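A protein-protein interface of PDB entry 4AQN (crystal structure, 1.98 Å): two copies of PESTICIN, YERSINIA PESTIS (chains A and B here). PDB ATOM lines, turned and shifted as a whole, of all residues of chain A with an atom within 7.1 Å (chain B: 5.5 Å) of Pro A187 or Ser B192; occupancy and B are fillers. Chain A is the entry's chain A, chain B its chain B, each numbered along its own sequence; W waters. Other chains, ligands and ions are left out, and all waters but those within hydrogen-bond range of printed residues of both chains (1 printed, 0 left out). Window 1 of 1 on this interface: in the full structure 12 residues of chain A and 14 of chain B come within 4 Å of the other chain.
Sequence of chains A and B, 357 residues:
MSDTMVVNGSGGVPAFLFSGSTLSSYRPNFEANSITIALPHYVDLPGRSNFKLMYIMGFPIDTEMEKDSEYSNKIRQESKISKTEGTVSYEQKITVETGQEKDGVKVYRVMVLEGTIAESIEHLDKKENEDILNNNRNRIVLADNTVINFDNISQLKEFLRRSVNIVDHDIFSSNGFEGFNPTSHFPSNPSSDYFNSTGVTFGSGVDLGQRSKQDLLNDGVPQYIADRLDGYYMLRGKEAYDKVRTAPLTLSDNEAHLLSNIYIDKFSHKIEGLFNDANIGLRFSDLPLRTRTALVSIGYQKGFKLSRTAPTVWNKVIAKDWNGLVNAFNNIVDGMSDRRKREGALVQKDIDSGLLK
Among the printed residues, merely in contact across the chains: Pro A187 with Asn B189 (3.5 Å), Pro A187 with Ser B191 (3.7 Å), Ser A188 with Asn B189 (3.3 Å), Asn A189 with Asn B189 (3.9 Å), Gly A335 with Asp B193 (3.6 Å), Gly A335 with Tyr B194 (3.5 Å) and Met A336 with Tyr B194 (3.9 Å).
OG of Ser B192 is in hydrogen-bond range of O of Pro A187 (3.2 Å). O of Ser B188 sits at hydrogen-bond distance from ND2 of Asn A189, 3.3 Å away. The side-chain hydroxyl of Tyr A194 sits at hydrogen-bond distance from the side-chain hydroxyl of Tyr B194 (3.1 Å). The side-chain carboxylate of Asp B193 sits at hydrogen-bond distance from the side-chain amide nitrogen of Gln A301. The side-chain carboxylate (OD2) of Asp B193 lies close to the side-chain sulfur (SD) of Met A336 (3.6 Å).
OG of Ser A188 lies within hydrogen-bond range of OG of Ser A192, 3.1 Å away. OD1 of Asn A189 is in hydrogen-bond range of N of Ser A192. The side-chain hydroxyl of Ser A192 lies close to the backbone NH of Tyr A194, at 3.2 Å. The side-chain amide oxygen of Gln A301 sits close to the side-chain sulfur of Met A336, at 3.5 Å. The side-chain hydroxyl of Ser B191 sits at hydrogen-bond distance from the side-chain amide oxygen of Asn B189. The side-chain amide nitrogen (ND2) of Asn B189 is in hydrogen-bond range of the side-chain hydroxyl (OG) of Ser B192 (2.7 Å).
Of the 16 printed residues of chain A, 7 touch a printed residue of chain B. Printed residues of chain B that touch a printed residue of chain A: Ser B188, Asn B189, Ser B191, Ser B192, Asp B193 and Tyr B194. Hydrophobic or aromatic side chains of chain B within 4 Å of the printed part of chain A: Tyr B194. Among the printed residues, no Asp or Glu carboxylate lies within 4 Å of a Lys or Arg side-chain nitrogen of the other chain.
Ser B192 touches one residue of chain A. Of the printed residues of chain A, Ser B188 touches Asn A189. Of the printed residues of chain B, Gly A335 touches Asp B193 (3.6 Å) and Tyr B194 (3.5 Å). Printed residues of chain A within 4 Å of Ser B191: Pro A187. Printed residues of chain B within 4 Å of Gln A301: Asp B193. Of the printed residues of chain B, Asn A189 touches Ser B188 and Asn B189.
Ser A188 touches Asn B189, and with the chains exchanged Asn A189 touches Ser B188. Asn B189 touches its own counterpart, Asn A189. Tyr B194 touches its own counterpart, Tyr A194. Of the 12 pairs that touch across the chains among the printed residues, 4 have their exchanged pair printed and touching as well.
Water W1 lies within hydrogen-bond range of the backbone carbonyl oxygen of Asp B193 and the side-chain amide nitrogen of Gln A301.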
ATOM      1  N   HIS A 185       1.163  27.138  17.964  1.00  0.00           N
ATOM      2  CA  HIS A 185       0.901  26.314  16.789  1.00  0.00           C
ATOM      3  C   HIS A 185      -0.233  25.317  17.016  1.00  0.00           C
ATOM      4  O   HIS A 185      -0.575  24.996  18.142  1.00  0.00           O
ATOM      5  CB  HIS A 185       2.195  25.625  16.291  1.00  0.00           C
ATOM      6  CG  HIS A 185       2.911  24.812  17.334  1.00  0.00           C
ATOM      7  ND1 HIS A 185       3.862  25.346  18.174  1.00  0.00           N
ATOM      8  CD2 HIS A 185       2.844  23.489  17.639  1.00  0.00           C
ATOM      9  CE1 HIS A 185       4.332  24.401  18.972  1.00  0.00           C
ATOM     10  NE2 HIS A 185       3.733  23.265  18.661  1.00  0.00           N
ATOM     11  N   PHE A 186      -0.851  24.880  15.930  1.00  0.00           N
ATOM     12  CA  PHE A 186      -1.954  23.938  15.996  1.00  0.00           C
ATOM     13  C   PHE A 186      -1.588  22.720  15.145  1.00  0.00           C
ATOM     14  O   PHE A 186      -1.736  22.737  13.919  1.00  0.00           O
ATOM     15  CB  PHE A 186      -3.220  24.601  15.475  1.00  0.00           C
ATOM     16  CG  PHE A 186      -4.432  23.735  15.561  1.00  0.00           C
ATOM     17  CD1 PHE A 186      -5.121  23.611  16.757  1.00  0.00           C
ATOM     18  CD2 PHE A 186      -4.890  23.045  14.447  1.00  0.00           C
ATOM     19  CE1 PHE A 186      -6.233  22.811  16.845  1.00  0.00           C
ATOM     20  CE2 PHE A 186      -6.010  22.241  14.525  1.00  0.00           C
ATOM     21  CZ  PHE A 186      -6.685  22.123  15.727  1.00  0.00           C
ATOM     22  N   PRO A 187      -1.094  21.657  15.792  1.00  0.00           N
ATOM     23  CA  PRO A 187      -0.497  20.572  15.005  1.00  0.00           C
ATOM     24  C   PRO A 187      -1.526  19.558  14.499  1.00  0.00           C
ATOM     25  O   PRO A 187      -1.302  18.343  14.568  1.00  0.00           O
ATOM     26  CB  PRO A 187       0.479  19.926  15.991  1.00  0.00           C
ATOM     27  CG  PRO A 187      -0.142  20.173  17.336  1.00  0.00           C
ATOM     28  CD  PRO A 187      -0.851  21.504  17.239  1.00  0.00           C
ATOM     29  N   SER A 188      -2.641  20.066  13.989  1.00  0.00           N
ATOM     30  CA  SER A 188      -3.635  19.232  13.314  1.00  0.00           C
ATOM     31  C   SER A 188      -4.282  20.002  12.175  1.00  0.00           C
ATOM     32  O   SER A 188      -4.008  21.188  11.994  1.00  0.00           O
ATOM     33  CB  SER A 188      -4.699  18.779  14.307  1.00  0.00           C
ATOM     34  OG  SER A 188      -5.408  17.673  13.812  1.00  0.00           O
ATOM     35  N   ASN A 189      -5.138  19.327  11.404  1.00  0.00           N
ATOM     36  CA  ASN A 189      -5.949  19.987  10.375  1.00  0.00           C
ATOM     37  C   ASN A 189      -7.385  19.439  10.417  1.00  0.00           C
ATOM     38  O   ASN A 189      -7.614  18.398  11.031  1.00  0.00           O
ATOM     39  CB  ASN A 189      -5.302  19.867   8.974  1.00  0.00           C
ATOM     40  CG  ASN A 189      -5.111  18.422   8.519  1.00  0.00           C
ATOM     41  OD1 ASN A 189      -5.570  17.478   9.166  1.00  0.00           O
ATOM     42  ND2 ASN A 189      -4.430  18.249   7.387  1.00  0.00           N
ATOM     43  N   SER A 192      -8.035  15.863   9.918  1.00  0.00           N
ATOM     44  CA  SER A 192      -7.443  14.970  10.907  1.00  0.00           C
ATOM     45  C   SER A 192      -8.449  14.479  11.953  1.00  0.00           C
ATOM     46  O   SER A 192      -9.466  15.129  12.236  1.00  0.00           O
ATOM     47  CB  SER A 192      -6.254  15.641  11.590  1.00  0.00           C
ATOM     48  OG  SER A 192      -5.752  14.843  12.647  1.00  0.00           O
ATOM     49  N   TYR A 194      -7.754  14.031  15.070  1.00  0.00           N
ATOM     50  CA  TYR A 194      -7.479  14.656  16.352  1.00  0.00           C
ATOM     51  C   TYR A 194      -7.807  16.141  16.350  1.00  0.00           C
ATOM     52  O   TYR A 194      -7.510  16.838  17.316  1.00  0.00           O
ATOM     53  CB  TYR A 194      -6.025  14.423  16.751  1.00  0.00           C
ATOM     54  CG  TYR A 194      -5.700  12.964  16.818  1.00  0.00           C
ATOM     55  CD1 TYR A 194      -6.148  12.192  17.877  1.00  0.00           C
ATOM     56  CD2 TYR A 194      -4.982  12.345  15.803  1.00  0.00           C
ATOM     57  CE1 TYR A 194      -5.868  10.851  17.943  1.00  0.00           C
ATOM     58  CE2 TYR A 194      -4.698  11.005  15.857  1.00  0.00           C
ATOM     59  CZ  TYR A 194      -5.142  10.262  16.935  1.00  0.00           C
ATOM     60  OH  TYR A 194      -4.868   8.920  17.009  1.00  0.00           O
ATOM     61  N   THR A 198      -7.276  18.749  19.697  1.00  0.00           N
ATOM     62  CA  THR A 198      -6.041  19.525  19.657  1.00  0.00           C
ATOM     63  C   THR A 198      -6.289  20.979  20.085  1.00  0.00           C
ATOM     64  O   THR A 198      -7.275  21.590  19.680  1.00  0.00           O
ATOM     65  CB  THR A 198      -5.415  19.478  18.264  1.00  0.00           C
ATOM     66  OG1 THR A 198      -5.213  18.113  17.893  1.00  0.00           O
ATOM     67  CG2 THR A 198      -4.065  20.193  18.255  1.00  0.00           C
ATOM     68  N   GLY A 199      -5.389  21.516  20.913  1.00  0.00           N
ATOM     69  CA  GLY A 199      -5.486  22.894  21.370  1.00  0.00           C
ATOM     70  C   GLY A 199      -4.263  23.702  20.970  1.00  0.00           C
ATOM     71  O   GLY A 199      -3.362  23.194  20.293  1.00  0.00           O
ATOM     72  N   VAL A 200      -4.215  24.964  21.397  1.00  0.00           N
ATOM     73  CA  VAL A 200      -3.108  25.838  21.017  1.00  0.00           C
ATOM     74  C   VAL A 200      -1.832  25.341  21.666  1.00  0.00           C
ATOM     75  O   VAL A 200      -1.803  25.076  22.870  1.00  0.00           O
ATOM     76  CB  VAL A 200      -3.358  27.277  21.464  1.00  0.00           C
ATOM     77  CG1 VAL A 200      -2.167  28.145  21.088  1.00  0.00           C
ATOM     78  CG2 VAL A 200      -4.654  27.803  20.844  1.00  0.00           C
ATOM     79  N   THR A 201      -0.762  25.210  20.892  1.00  0.00           N
ATOM     80  CA  THR A 201       0.410  24.543  21.446  1.00  0.00           C
ATOM     81  C   THR A 201       1.660  25.439  21.414  1.00  0.00           C
ATOM     82  O   THR A 201       1.856  26.194  20.465  1.00  0.00           O
ATOM     83  CB  THR A 201       0.634  23.193  20.723  1.00  0.00           C
ATOM     84  OG1 THR A 201      -0.588  22.430  20.754  1.00  0.00           O
ATOM     85  CG2 THR A 201       1.754  22.393  21.403  1.00  0.00           C
ATOM     86  N   GLY A 205       5.361  20.688  22.614  1.00  0.00           N
ATOM     87  CA  GLY A 205       4.105  20.020  22.916  1.00  0.00           C
ATOM     88  C   GLY A 205       3.354  20.500  24.146  1.00  0.00           C
ATOM     89  O   GLY A 205       2.620  19.721  24.759  1.00  0.00           O
ATOM     90  N   ASP A 207       0.283  21.908  25.299  1.00  0.00           N
ATOM     91  CA  ASP A 207      -1.038  22.106  24.719  1.00  0.00           C
ATOM     92  C   ASP A 207      -1.956  22.699  25.790  1.00  0.00           C
ATOM     93  O   ASP A 207      -2.113  22.124  26.874  1.00  0.00           O
ATOM     94  CB  ASP A 207      -1.557  20.735  24.234  1.00  0.00           C
ATOM     95  CG  ASP A 207      -2.911  20.802  23.506  1.00  0.00           C
ATOM     96  OD1 ASP A 207      -3.855  21.468  23.998  1.00  0.00           O
ATOM     97  OD2 ASP A 207      -3.041  20.148  22.428  1.00  0.00           O
ATOM     98  N   GLN A 301       3.875  10.839  23.907  1.00  0.00           N
ATOM     99  CA  GLN A 301       3.198  10.855  22.622  1.00  0.00           C
ATOM    100  C   GLN A 301       2.004   9.901  22.609  1.00  0.00           C
ATOM    101  O   GLN A 301       0.949  10.237  22.063  1.00  0.00           O
ATOM    102  CB  GLN A 301       4.182  10.533  21.480  1.00  0.00           C
ATOM    103  CG  GLN A 301       3.613  10.760  20.077  1.00  0.00           C
ATOM    104  CD  GLN A 301       4.645  10.584  18.959  1.00  0.00           C
ATOM    105  OE1 GLN A 301       5.354   9.580  18.904  1.00  0.00           O
ATOM    106  NE2 GLN A 301       4.722  11.564  18.058  1.00  0.00           N
ATOM    107  N   GLY A 335       2.011   3.987  12.927  1.00  0.00           N
ATOM    108  CA  GLY A 335       1.979   5.199  12.127  1.00  0.00           C
ATOM    109  C   GLY A 335       3.016   6.221  12.569  1.00  0.00           C
ATOM    110  O   GLY A 335       3.089   7.324  12.024  1.00  0.00           O
ATOM    111  N   MET A 336       3.807   5.861  13.573  1.00  0.00           N
ATOM    112  CA  MET A 336       4.844   6.736  14.100  1.00  0.00           C
ATOM    113  C   MET A 336       6.173   5.986  14.203  1.00  0.00           C
ATOM    114  O   MET A 336       6.967   6.235  15.124  1.00  0.00           O
ATOM    115  CB  MET A 336       4.445   7.255  15.489  1.00  0.00           C
ATOM    116  CG  MET A 336       3.243   8.180  15.510  1.00  0.00           C
ATOM    117  SD  MET A 336       2.536   8.367  17.165  1.00  0.00           S
ATOM    118  CE  MET A 336       1.784   6.743  17.382  1.00  0.00           C
ATOM    119  N   SER B 188      -3.013  14.834   7.175  1.00  0.00           N
ATOM    120  CA  SER B 188      -2.065  15.096   8.251  1.00  0.00           C
ATOM    121  C   SER B 188      -1.235  16.328   7.914  1.00  0.00           C
ATOM    122  O   SER B 188      -1.471  16.992   6.895  1.00  0.00           O
ATOM    123  CB  SER B 188      -1.161  13.883   8.511  1.00  0.00           C
ATOM    124  OG  SER B 188      -0.190  14.169   9.507  1.00  0.00           O
ATOM    125  N   ASN B 189      -0.277  16.643   8.781  1.00  0.00           N
ATOM    126  CA  ASN B 189       0.640  17.762   8.563  1.00  0.00           C
ATOM    127  C   ASN B 189       1.994  17.406   9.189  1.00  0.00           C
ATOM    128  O   ASN B 189       2.054  16.521  10.052  1.00  0.00           O
ATOM    129  CB  ASN B 189       0.052  19.063   9.131  1.00  0.00           C
ATOM    130  CG  ASN B 189      -0.159  19.004  10.634  1.00  0.00           C
ATOM    131  OD1 ASN B 189       0.710  19.405  11.411  1.00  0.00           O
ATOM    132  ND2 ASN B 189      -1.319  18.500  11.049  1.00  0.00           N
ATOM    133  N   PRO B 190       3.085  18.054   8.737  1.00  0.00           N
ATOM    134  CA  PRO B 190       4.448  17.692   9.159  1.00  0.00           C
ATOM    135  C   PRO B 190       4.666  17.604  10.672  1.00  0.00           C
ATOM    136  O   PRO B 190       5.434  16.746  11.114  1.00  0.00           O
ATOM    137  CB  PRO B 190       5.299  18.807   8.560  1.00  0.00           C
ATOM    138  CG  PRO B 190       4.562  19.191   7.324  1.00  0.00           C
ATOM    139  CD  PRO B 190       3.101  19.092   7.686  1.00  0.00           C
ATOM    140  N   SER B 191       4.008  18.467  11.443  1.00  0.00           N
ATOM    141  CA  SER B 191       4.143  18.444  12.898  1.00  0.00           C
ATOM    142  C   SER B 191       3.700  17.098  13.451  1.00  0.00           C
ATOM    143  O   SER B 191       4.457  16.405  14.135  1.00  0.00           O
ATOM    144  CB  SER B 191       3.289  19.542  13.541  1.00  0.00           C
ATOM    145  OG  SER B 191       2.937  20.547  12.611  1.00  0.00           O
ATOM    146  N   SER B 192       2.465  16.739  13.118  1.00  0.00           N
ATOM    147  CA  SER B 192       1.769  15.600  13.707  1.00  0.00           C
ATOM    148  C   SER B 192       2.537  14.285  13.730  1.00  0.00           C
ATOM    149  O   SER B 192       3.453  14.050  12.931  1.00  0.00           O
ATOM    150  CB  SER B 192       0.432  15.378  13.004  1.00  0.00           C
ATOM    151  OG  SER B 192       0.060  16.524  12.266  1.00  0.00           O
ATOM    152  N   ASP B 193       2.120  13.447  14.673  1.00  0.00           N
ATOM    153  CA  ASP B 193       2.647  12.112  14.909  1.00  0.00           C
ATOM    154  C   ASP B 193       2.728  11.264  13.643  1.00  0.00           C
ATOM    155  O   ASP B 193       3.696  10.536  13.429  1.00  0.00           O
ATOM    156  CB  ASP B 193       1.730  11.400  15.908  1.00  0.00           C
ATOM    157  CG  ASP B 193       1.668  12.099  17.267  1.00  0.00           C
ATOM    158  OD1 ASP B 193       2.231  13.212  17.408  1.00  0.00           O
ATOM    159  OD2 ASP B 193       1.047  11.524  18.195  1.00  0.00           O
ATOM    160  N   TYR B 194       1.705  11.371  12.804  1.00  0.00           N
ATOM    161  CA  TYR B 194       1.516  10.427  11.709  1.00  0.00           C
ATOM    162  C   TYR B 194       1.935  10.941  10.335  1.00  0.00           C
ATOM    163  O   TYR B 194       1.642  10.304   9.327  1.00  0.00           O
ATOM    164  CB  TYR B 194       0.052  10.001  11.666  1.00  0.00           C
ATOM    165  CG  TYR B 194      -0.456   9.486  12.986  1.00  0.00           C
ATOM    166  CD1 TYR B 194      -0.296   8.156  13.337  1.00  0.00           C
ATOM    167  CD2 TYR B 194      -1.097  10.335  13.882  1.00  0.00           C
ATOM    168  CE1 TYR B 194      -0.764   7.676  14.541  1.00  0.00           C
ATOM    169  CE2 TYR B 194      -1.565   9.870  15.090  1.00  0.00           C
ATOM    170  CZ  TYR B 194      -1.399   8.540  15.412  1.00  0.00           C
ATOM    171  OH  TYR B 194      -1.868   8.073  16.615  1.00  0.00           O
ATOM    172  N   PHE B 195       2.618  12.079  10.293  1.00  0.00           N
ATOM    173  CA  PHE B 195       3.007  12.690   9.019  1.00  0.00           C
ATOM    174  C   PHE B 195       3.651  11.714   8.039  1.00  0.00           C
ATOM    175  O   PHE B 195       3.362  11.748   6.846  1.00  0.00           O
ATOM    176  CB  PHE B 195       3.949  13.870   9.234  1.00  0.00           C
ATOM    177  CG  PHE B 195       4.443  14.490   7.948  1.00  0.00           C
ATOM    178  CD1 PHE B 195       3.577  15.195   7.118  1.00  0.00           C
ATOM    179  CD2 PHE B 195       5.772  14.365   7.567  1.00  0.00           C
ATOM    180  CE1 PHE B 195       4.032  15.777   5.940  1.00  0.00           C
ATOM    181  CE2 PHE B 195       6.232  14.943   6.387  1.00  0.00           C
ATOM    182  CZ  PHE B 195       5.360  15.645   5.576  1.00  0.00           C
HETATM  183  O   HOH W   1       5.612  10.448  14.898  1.00  0.00           O
